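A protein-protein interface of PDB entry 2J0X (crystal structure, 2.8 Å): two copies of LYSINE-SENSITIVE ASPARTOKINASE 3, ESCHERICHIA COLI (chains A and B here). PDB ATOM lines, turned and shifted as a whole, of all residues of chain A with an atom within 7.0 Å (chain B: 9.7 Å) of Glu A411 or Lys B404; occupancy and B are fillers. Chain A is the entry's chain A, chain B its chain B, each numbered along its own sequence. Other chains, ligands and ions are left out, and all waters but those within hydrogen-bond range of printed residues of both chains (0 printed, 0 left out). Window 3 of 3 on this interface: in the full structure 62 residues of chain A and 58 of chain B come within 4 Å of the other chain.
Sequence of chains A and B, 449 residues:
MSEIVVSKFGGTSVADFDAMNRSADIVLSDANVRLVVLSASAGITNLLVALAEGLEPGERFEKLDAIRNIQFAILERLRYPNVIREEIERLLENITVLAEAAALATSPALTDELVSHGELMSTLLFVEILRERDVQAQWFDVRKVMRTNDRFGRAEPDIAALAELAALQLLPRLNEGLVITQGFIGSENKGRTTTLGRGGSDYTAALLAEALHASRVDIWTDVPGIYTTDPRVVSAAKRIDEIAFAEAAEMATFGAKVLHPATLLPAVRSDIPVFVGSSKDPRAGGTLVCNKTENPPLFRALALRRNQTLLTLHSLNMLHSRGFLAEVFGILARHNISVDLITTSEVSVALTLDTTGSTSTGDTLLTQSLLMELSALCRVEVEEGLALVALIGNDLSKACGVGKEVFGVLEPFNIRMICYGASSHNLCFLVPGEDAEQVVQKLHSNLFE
The side-chain carboxylate (OE2) of Glu A411 lies within salt-bridge range of the side-chain amino group (NZ) of Lys B404, at 3.0 Å. The side-chain amide oxygen of Asn A414 lies within hydrogen-bond range of the backbone NH of Gly B403, 3.1 Å away. The backbone carbonyl oxygen of Val B402 is in hydrogen-bond range of the backbone NH of Ile A415 (2.8 Å).
Positions printed for both chains: 407, 408, 409, 410, 411 and 412. Of the 12 pairs that touch across the chains among the printed residues, none has its exchanged pair printed and touching as well.
Of chain B, only Lys B404 comes within 4 Å of Glu A411. Printed residues of chain B within 4 Å of Pro A412: Lys B404. Of the printed residues of chain B, Asn A414 touches Gly B401 (3.7 Å), Val B402 (3.2 Å) and Gly B403 (3.1 Å). Printed residues of chain A within 4 Å of Gly B403: Phe A413 (3.7 Å) and Asn A414 (3.1 Å). Lys B404 touches just these residues of chain A: Glu A411 and Pro A412. Of the printed residues of chain A, Phe B407 touches Phe A413 (3.8 Å) and Ile A415 (3.3 Å). The nearest residue of chain B that does not touch Glu A411 is Gly B403 (4.7 Å).
The backbone NH (N) of Gly B403 lies within hydrogen-bond range of the side-chain carboxylate (OE1) of Glu B405 (3.1 Å).
Printed residues of chain A that touch a printed residue of chain B: Glu A411, Pro A412, Phe A413, Asn A414 and Ile A415. Among the printed residues, 12 pairs touch across the chains.
CA of Pro A412 touches NZ of Lys B404, at 3.4 Å. Phe A413 touches Val B402. O of Phe A413 touches CA of Gly B403, 3.7 Å away. CE1 of Phe B407 touches O of Phe A413 (3.8 Å). CB of Asn A414 touches C of Gly B401, 3.7 Å away. Asn A414 touches Val B402. Ile A415 touches Gly B401. Ile A415 touches Phe B407 (CD1 to CE1, 3.3 Å). Ile A415 touches Tyr B420 (O to CE2, 3.4 Å).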
ATOM      1  N   PHE A 407     -25.079  -2.865  31.705  1.00  0.00           N
ATOM      2  CA  PHE A 407     -24.463  -4.008  31.032  1.00  0.00           C
ATOM      3  C   PHE A 407     -24.219  -3.849  29.534  1.00  0.00           C
ATOM      4  O   PHE A 407     -23.122  -4.131  29.045  1.00  0.00           O
ATOM      5  CB  PHE A 407     -25.311  -5.261  31.277  1.00  0.00           C
ATOM      6  CG  PHE A 407     -25.446  -5.628  32.729  1.00  0.00           C
ATOM      7  CD1 PHE A 407     -26.391  -6.565  33.133  1.00  0.00           C
ATOM      8  CD2 PHE A 407     -24.637  -5.027  33.695  1.00  0.00           C
ATOM      9  CE1 PHE A 407     -26.529  -6.895  34.478  1.00  0.00           C
ATOM     10  CE2 PHE A 407     -24.766  -5.348  35.041  1.00  0.00           C
ATOM     11  CZ  PHE A 407     -25.713  -6.282  35.436  1.00  0.00           C
ATOM     12  N   GLY A 408     -25.244  -3.406  28.813  1.00  0.00           N
ATOM     13  CA  GLY A 408     -25.129  -3.229  27.375  1.00  0.00           C
ATOM     14  C   GLY A 408     -23.832  -2.571  26.955  1.00  0.00           C
ATOM     15  O   GLY A 408     -23.336  -2.788  25.850  1.00  0.00           O
ATOM     16  N   VAL A 409     -23.272  -1.772  27.849  1.00  0.00           N
ATOM     17  CA  VAL A 409     -22.037  -1.072  27.564  1.00  0.00           C
ATOM     18  C   VAL A 409     -20.903  -2.003  27.147  1.00  0.00           C
ATOM     19  O   VAL A 409     -20.065  -1.630  26.328  1.00  0.00           O
ATOM     20  CB  VAL A 409     -21.586  -0.258  28.789  1.00  0.00           C
ATOM     21  CG1 VAL A 409     -22.668   0.749  29.177  1.00  0.00           C
ATOM     22  CG2 VAL A 409     -21.292  -1.193  29.943  1.00  0.00           C
ATOM     23  N   LEU A 410     -20.900  -3.217  27.695  1.00  0.00           N
ATOM     24  CA  LEU A 410     -19.853  -4.206  27.427  1.00  0.00           C
ATOM     25  C   LEU A 410     -20.238  -5.261  26.388  1.00  0.00           C
ATOM     26  O   LEU A 410     -19.579  -6.295  26.270  1.00  0.00           O
ATOM     27  CB  LEU A 410     -19.495  -4.934  28.735  1.00  0.00           C
ATOM     28  CG  LEU A 410     -19.510  -4.198  30.084  1.00  0.00           C
ATOM     29  CD1 LEU A 410     -19.242  -5.194  31.188  1.00  0.00           C
ATOM     30  CD2 LEU A 410     -18.470  -3.097  30.115  1.00  0.00           C
ATOM     31  N   GLU A 411     -21.293  -5.007  25.635  1.00  0.00           N
ATOM     32  CA  GLU A 411     -21.753  -5.977  24.655  1.00  0.00           C
ATOM     33  C   GLU A 411     -20.804  -6.306  23.503  1.00  0.00           C
ATOM     34  O   GLU A 411     -20.445  -7.468  23.290  1.00  0.00           O
ATOM     35  CB  GLU A 411     -23.089  -5.521  24.080  1.00  0.00           C
ATOM     36  CG  GLU A 411     -23.624  -6.444  23.023  1.00  0.00           C
ATOM     37  CD  GLU A 411     -24.890  -5.922  22.395  1.00  0.00           C
ATOM     38  OE1 GLU A 411     -25.863  -5.670  23.141  1.00  0.00           O
ATOM     39  OE2 GLU A 411     -24.910  -5.767  21.155  1.00  0.00           O
ATOM     40  N   PRO A 412     -20.382  -5.288  22.748  1.00  0.00           N
ATOM     41  CA  PRO A 412     -19.481  -5.468  21.607  1.00  0.00           C
ATOM     42  C   PRO A 412     -18.107  -6.081  21.814  1.00  0.00           C
ATOM     43  O   PRO A 412     -17.360  -6.223  20.850  1.00  0.00           O
ATOM     44  CB  PRO A 412     -19.383  -4.062  21.029  1.00  0.00           C
ATOM     45  CG  PRO A 412     -19.515  -3.203  22.231  1.00  0.00           C
ATOM     46  CD  PRO A 412     -20.654  -3.858  22.969  1.00  0.00           C
ATOM     47  N   PHE A 413     -17.762  -6.474  23.034  1.00  0.00           N
ATOM     48  CA  PHE A 413     -16.428  -7.023  23.245  1.00  0.00           C
ATOM     49  C   PHE A 413     -16.341  -8.453  23.742  1.00  0.00           C
ATOM     50  O   PHE A 413     -17.289  -8.982  24.324  1.00  0.00           O
ATOM     51  CB  PHE A 413     -15.667  -6.116  24.197  1.00  0.00           C
ATOM     52  CG  PHE A 413     -16.094  -4.688  24.119  1.00  0.00           C
ATOM     53  CD1 PHE A 413     -17.177  -4.235  24.868  1.00  0.00           C
ATOM     54  CD2 PHE A 413     -15.443  -3.799  23.271  1.00  0.00           C
ATOM     55  CE1 PHE A 413     -17.605  -2.915  24.776  1.00  0.00           C
ATOM     56  CE2 PHE A 413     -15.864  -2.482  23.172  1.00  0.00           C
ATOM     57  CZ  PHE A 413     -16.948  -2.039  23.927  1.00  0.00           C
ATOM     58  N   ASN A 414     -15.191  -9.075  23.490  1.00  0.00           N
ATOM     59  CA  ASN A 414     -14.939 -10.440  23.933  1.00  0.00           C
ATOM     60  C   ASN A 414     -14.329 -10.302  25.311  1.00  0.00           C
ATOM     61  O   ASN A 414     -13.189  -9.876  25.467  1.00  0.00           O
ATOM     62  CB  ASN A 414     -13.975 -11.149  22.987  1.00  0.00           C
ATOM     63  CG  ASN A 414     -14.522 -11.243  21.592  1.00  0.00           C
ATOM     64  OD1 ASN A 414     -15.670 -11.651  21.392  1.00  0.00           O
ATOM     65  ND2 ASN A 414     -13.711 -10.863  20.610  1.00  0.00           N
ATOM     66  N   ILE A 415     -15.114 -10.655  26.312  1.00  0.00           N
ATOM     67  CA  ILE A 415     -14.686 -10.523  27.681  1.00  0.00           C
ATOM     68  C   ILE A 415     -14.236 -11.860  28.238  1.00  0.00           C
ATOM     69  O   ILE A 415     -14.879 -12.881  28.003  1.00  0.00           O
ATOM     70  CB  ILE A 415     -15.848  -9.924  28.489  1.00  0.00           C
ATOM     71  CG1 ILE A 415     -16.386  -8.696  27.729  1.00  0.00           C
ATOM     72  CG2 ILE A 415     -15.387  -9.556  29.883  1.00  0.00           C
ATOM     73  CD1 ILE A 415     -17.590  -8.029  28.351  1.00  0.00           C
ATOM     74  N   LEU B 298     -23.363 -25.386  23.773  1.00  0.00           N
ATOM     75  CA  LEU B 298     -22.905 -24.122  24.337  1.00  0.00           C
ATOM     76  C   LEU B 298     -23.490 -24.019  25.730  1.00  0.00           C
ATOM     77  O   LEU B 298     -22.838 -23.555  26.668  1.00  0.00           O
ATOM     78  CB  LEU B 298     -23.400 -22.944  23.505  1.00  0.00           C
ATOM     79  CG  LEU B 298     -23.109 -21.602  24.172  1.00  0.00           C
ATOM     80  CD1 LEU B 298     -21.612 -21.473  24.446  1.00  0.00           C
ATOM     81  CD2 LEU B 298     -23.590 -20.481  23.284  1.00  0.00           C
ATOM     82  N   PHE B 299     -24.741 -24.449  25.840  1.00  0.00           N
ATOM     83  CA  PHE B 299     -25.449 -24.458  27.110  1.00  0.00           C
ATOM     84  C   PHE B 299     -26.014 -25.850  27.362  1.00  0.00           C
ATOM     85  O   PHE B 299     -26.720 -26.405  26.523  1.00  0.00           O
ATOM     86  CB  PHE B 299     -26.576 -23.430  27.108  1.00  0.00           C
ATOM     87  CG  PHE B 299     -26.091 -22.013  27.187  1.00  0.00           C
ATOM     88  CD1 PHE B 299     -26.106 -21.194  26.070  1.00  0.00           C
ATOM     89  CD2 PHE B 299     -25.588 -21.506  28.381  1.00  0.00           C
ATOM     90  CE1 PHE B 299     -25.626 -19.892  26.143  1.00  0.00           C
ATOM     91  CE2 PHE B 299     -25.107 -20.211  28.461  1.00  0.00           C
ATOM     92  CZ  PHE B 299     -25.125 -19.402  27.339  1.00  0.00           C
ATOM     93  N   LEU B 396     -17.757 -21.482  27.288  1.00  0.00           N
ATOM     94  CA  LEU B 396     -18.269 -20.222  27.812  1.00  0.00           C
ATOM     95  C   LEU B 396     -17.158 -19.232  28.149  1.00  0.00           C
ATOM     96  O   LEU B 396     -17.435 -18.111  28.539  1.00  0.00           O
ATOM     97  CB  LEU B 396     -19.129 -20.489  29.048  1.00  0.00           C
ATOM     98  CG  LEU B 396     -20.257 -21.511  28.854  1.00  0.00           C
ATOM     99  CD1 LEU B 396     -21.063 -21.645  30.127  1.00  0.00           C
ATOM    100  CD2 LEU B 396     -21.164 -21.070  27.721  1.00  0.00           C
ATOM    101  N   GLY B 401     -11.254 -14.303  25.294  1.00  0.00           N
ATOM    102  CA  GLY B 401     -12.532 -13.785  25.739  1.00  0.00           C
ATOM    103  C   GLY B 401     -13.689 -14.311  24.913  1.00  0.00           C
ATOM    104  O   GLY B 401     -13.486 -14.970  23.900  1.00  0.00           O
ATOM    105  N   VAL B 402     -14.906 -14.016  25.352  1.00  0.00           N
ATOM    106  CA  VAL B 402     -16.112 -14.458  24.669  1.00  0.00           C
ATOM    107  C   VAL B 402     -16.998 -13.252  24.393  1.00  0.00           C
ATOM    108  O   VAL B 402     -17.124 -12.363  25.233  1.00  0.00           O
ATOM    109  CB  VAL B 402     -16.892 -15.477  25.538  1.00  0.00           C
ATOM    110  CG1 VAL B 402     -18.338 -15.036  25.716  1.00  0.00           C
ATOM    111  CG2 VAL B 402     -16.837 -16.848  24.898  1.00  0.00           C
ATOM    112  N   GLY B 403     -17.617 -13.236  23.218  1.00  0.00           N
ATOM    113  CA  GLY B 403     -18.474 -12.126  22.844  1.00  0.00           C
ATOM    114  C   GLY B 403     -19.841 -12.145  23.501  1.00  0.00           C
ATOM    115  O   GLY B 403     -20.022 -12.707  24.580  1.00  0.00           O
ATOM    116  N   LYS B 404     -20.803 -11.518  22.835  1.00  0.00           N
ATOM    117  CA  LYS B 404     -22.170 -11.435  23.328  1.00  0.00           C
ATOM    118  C   LYS B 404     -22.928 -12.751  23.154  1.00  0.00           C
ATOM    119  O   LYS B 404     -24.029 -12.919  23.689  1.00  0.00           O
ATOM    120  CB  LYS B 404     -22.893 -10.300  22.599  1.00  0.00           C
ATOM    121  CG  LYS B 404     -22.769 -10.373  21.079  1.00  0.00           C
ATOM    122  CD  LYS B 404     -23.040  -9.024  20.408  1.00  0.00           C
ATOM    123  CE  LYS B 404     -21.912  -8.020  20.657  1.00  0.00           C
ATOM    124  NZ  LYS B 404     -22.227  -6.668  20.101  1.00  0.00           N
ATOM    125  N   GLU B 405     -22.337 -13.683  22.406  1.00  0.00           N
ATOM    126  CA  GLU B 405     -22.969 -14.981  22.174  1.00  0.00           C
ATOM    127  C   GLU B 405     -23.311 -15.579  23.525  1.00  0.00           C
ATOM    128  O   GLU B 405     -24.366 -16.178  23.704  1.00  0.00           O
ATOM    129  CB  GLU B 405     -22.030 -15.946  21.444  1.00  0.00           C
ATOM    130  CG  GLU B 405     -21.423 -15.412  20.169  1.00  0.00           C
ATOM    131  CD  GLU B 405     -20.304 -14.431  20.431  1.00  0.00           C
ATOM    132  OE1 GLU B 405     -19.342 -14.806  21.135  1.00  0.00           O
ATOM    133  OE2 GLU B 405     -20.386 -13.291  19.931  1.00  0.00           O
ATOM    134  N   VAL B 406     -22.402 -15.399  24.475  1.00  0.00           N
ATOM    135  CA  VAL B 406     -22.576 -15.924  25.821  1.00  0.00           C
ATOM    136  C   VAL B 406     -23.165 -14.890  26.790  1.00  0.00           C
ATOM    137  O   VAL B 406     -23.811 -15.259  27.767  1.00  0.00           O
ATOM    138  CB  VAL B 406     -21.220 -16.443  26.379  1.00  0.00           C
ATOM    139  CG1 VAL B 406     -21.411 -17.096  27.729  1.00  0.00           C
ATOM    140  CG2 VAL B 406     -20.612 -17.430  25.409  1.00  0.00           C
ATOM    141  N   PHE B 407     -22.967 -13.601  26.518  1.00  0.00           N
ATOM    142  CA  PHE B 407     -23.475 -12.549  27.408  1.00  0.00           C
ATOM    143  C   PHE B 407     -24.918 -12.135  27.151  1.00  0.00           C
ATOM    144  O   PHE B 407     -25.716 -12.037  28.086  1.00  0.00           O
ATOM    145  CB  PHE B 407     -22.603 -11.298  27.307  1.00  0.00           C
ATOM    146  CG  PHE B 407     -21.151 -11.555  27.516  1.00  0.00           C
ATOM    147  CD1 PHE B 407     -20.208 -10.638  27.069  1.00  0.00           C
ATOM    148  CD2 PHE B 407     -20.718 -12.720  28.143  1.00  0.00           C
ATOM    149  CE1 PHE B 407     -18.855 -10.879  27.236  1.00  0.00           C
ATOM    150  CE2 PHE B 407     -19.367 -12.972  28.317  1.00  0.00           C
ATOM    151  CZ  PHE B 407     -18.430 -12.050  27.861  1.00  0.00           C
ATOM    152  N   GLY B 408     -25.242 -11.869  25.887  1.00  0.00           N
ATOM    153  CA  GLY B 408     -26.587 -11.447  25.536  1.00  0.00           C
ATOM    154  C   GLY B 408     -27.651 -12.245  26.265  1.00  0.00           C
ATOM    155  O   GLY B 408     -28.764 -11.772  26.496  1.00  0.00           O
ATOM    156  N   VAL B 409     -27.280 -13.466  26.629  1.00  0.00           N
ATOM    157  CA  VAL B 409     -28.151 -14.391  27.329  1.00  0.00           C
ATOM    158  C   VAL B 409     -28.820 -13.780  28.550  1.00  0.00           C
ATOM    159  O   VAL B 409     -29.998 -14.021  28.811  1.00  0.00           O
ATOM    160  CB  VAL B 409     -27.357 -15.619  27.795  1.00  0.00           C
ATOM    161  CG1 VAL B 409     -28.313 -16.725  28.201  1.00  0.00           C
ATOM    162  CG2 VAL B 409     -26.400 -16.070  26.690  1.00  0.00           C
ATOM    163  N   LEU B 410     -28.071 -12.996  29.314  1.00  0.00           N
ATOM    164  CA  LEU B 410     -28.655 -12.400  30.506  1.00  0.00           C
ATOM    165  C   LEU B 410     -28.930 -10.904  30.426  1.00  0.00           C
ATOM    166  O   LEU B 410     -28.914 -10.198  31.433  1.00  0.00           O
ATOM    167  CB  LEU B 410     -27.806 -12.737  31.744  1.00  0.00           C
ATOM    168  CG  LEU B 410     -26.278 -12.795  31.680  1.00  0.00           C
ATOM    169  CD1 LEU B 410     -25.690 -11.393  31.537  1.00  0.00           C
ATOM    170  CD2 LEU B 410     -25.766 -13.471  32.947  1.00  0.00           C
ATOM    171  N   GLU B 411     -29.217 -10.423  29.224  1.00  0.00           N
ATOM    172  CA  GLU B 411     -29.503  -9.009  29.040  1.00  0.00           C
ATOM    173  C   GLU B 411     -30.815  -8.585  29.698  1.00  0.00           C
ATOM    174  O   GLU B 411     -30.849  -7.640  30.490  1.00  0.00           O
ATOM    175  CB  GLU B 411     -29.570  -8.662  27.552  1.00  0.00           C
ATOM    176  CG  GLU B 411     -29.807  -7.180  27.288  1.00  0.00           C
ATOM    177  CD  GLU B 411     -30.896  -6.934  26.264  1.00  0.00           C
ATOM    178  OE1 GLU B 411     -31.092  -5.759  25.881  1.00  0.00           O
ATOM    179  OE2 GLU B 411     -31.554  -7.913  25.850  1.00  0.00           O
ATOM    180  N   PRO B 412     -31.912  -9.290  29.385  1.00  0.00           N
ATOM    181  CA  PRO B 412     -33.244  -8.998  29.923  1.00  0.00           C
ATOM    182  C   PRO B 412     -33.462  -8.972  31.435  1.00  0.00           C
ATOM    183  O   PRO B 412     -34.553  -8.627  31.883  1.00  0.00           O
ATOM    184  CB  PRO B 412     -34.116 -10.051  29.246  1.00  0.00           C
ATOM    185  CG  PRO B 412     -33.180 -11.200  29.084  1.00  0.00           C
ATOM    186  CD  PRO B 412     -31.942 -10.522  28.576  1.00  0.00           C
ATOM    187  N   TYR B 420     -17.750 -14.649  36.391  1.00  0.00           N
ATOM    188  CA  TYR B 420     -17.423 -15.213  35.097  1.00  0.00           C
ATOM    189  C   TYR B 420     -15.924 -15.157  34.797  1.00  0.00           C
ATOM    190  O   TYR B 420     -15.254 -14.174  35.103  1.00  0.00           O
ATOM    191  CB  TYR B 420     -18.211 -14.461  34.028  1.00  0.00           C
ATOM    192  CG  TYR B 420     -17.816 -14.829  32.633  1.00  0.00           C
ATOM    193  CD1 TYR B 420     -18.243 -16.025  32.061  1.00  0.00           C
ATOM    194  CD2 TYR B 420     -16.956 -14.008  31.903  1.00  0.00           C
ATOM    195  CE1 TYR B 420     -17.817 -16.398  30.796  1.00  0.00           C
ATOM    196  CE2 TYR B 420     -16.524 -14.368  30.644  1.00  0.00           C
ATOM    197  CZ  TYR B 420     -16.952 -15.566  30.094  1.00  0.00           C
ATOM    198  OH  TYR B 420     -16.485 -15.932  28.853  1.00  0.00           O
ATOM    199  N   LEU B 427     -21.196 -20.138  34.221  1.00  0.00           N
ATOM    200  CA  LEU B 427     -21.453 -18.708  34.198  1.00  0.00           C
ATOM    201  C   LEU B 427     -22.593 -18.536  35.185  1.00  0.00           C
ATOM    202  O   LEU B 427     -23.703 -18.995  34.926  1.00  0.00           O
ATOM    203  CB  LEU B 427     -21.929 -18.223  32.820  1.00  0.00           C
ATOM    204  CG  LEU B 427     -22.033 -16.693  32.593  1.00  0.00           C
ATOM    205  CD1 LEU B 427     -22.842 -16.425  31.336  1.00  0.00           C
ATOM    206  CD2 LEU B 427     -22.711 -15.994  33.762  1.00  0.00           C
ATOM    207  N   LEU B 447     -33.075 -20.867  25.579  1.00  0.00           N
ATOM    208  CA  LEU B 447     -31.862 -21.663  25.495  1.00  0.00           C
ATOM    209  C   LEU B 447     -32.140 -23.143  25.279  1.00  0.00           C
ATOM    210  O   LEU B 447     -31.352 -23.838  24.642  1.00  0.00           O
ATOM    211  CB  LEU B 447     -31.028 -21.500  26.769  1.00  0.00           C
ATOM    212  CG  LEU B 447     -29.972 -20.393  26.855  1.00  0.00           C
ATOM    213  CD1 LEU B 447     -30.650 -19.046  26.857  1.00  0.00           C
ATOM    214  CD2 LEU B 447     -29.137 -20.562  28.128  1.00  0.00           C
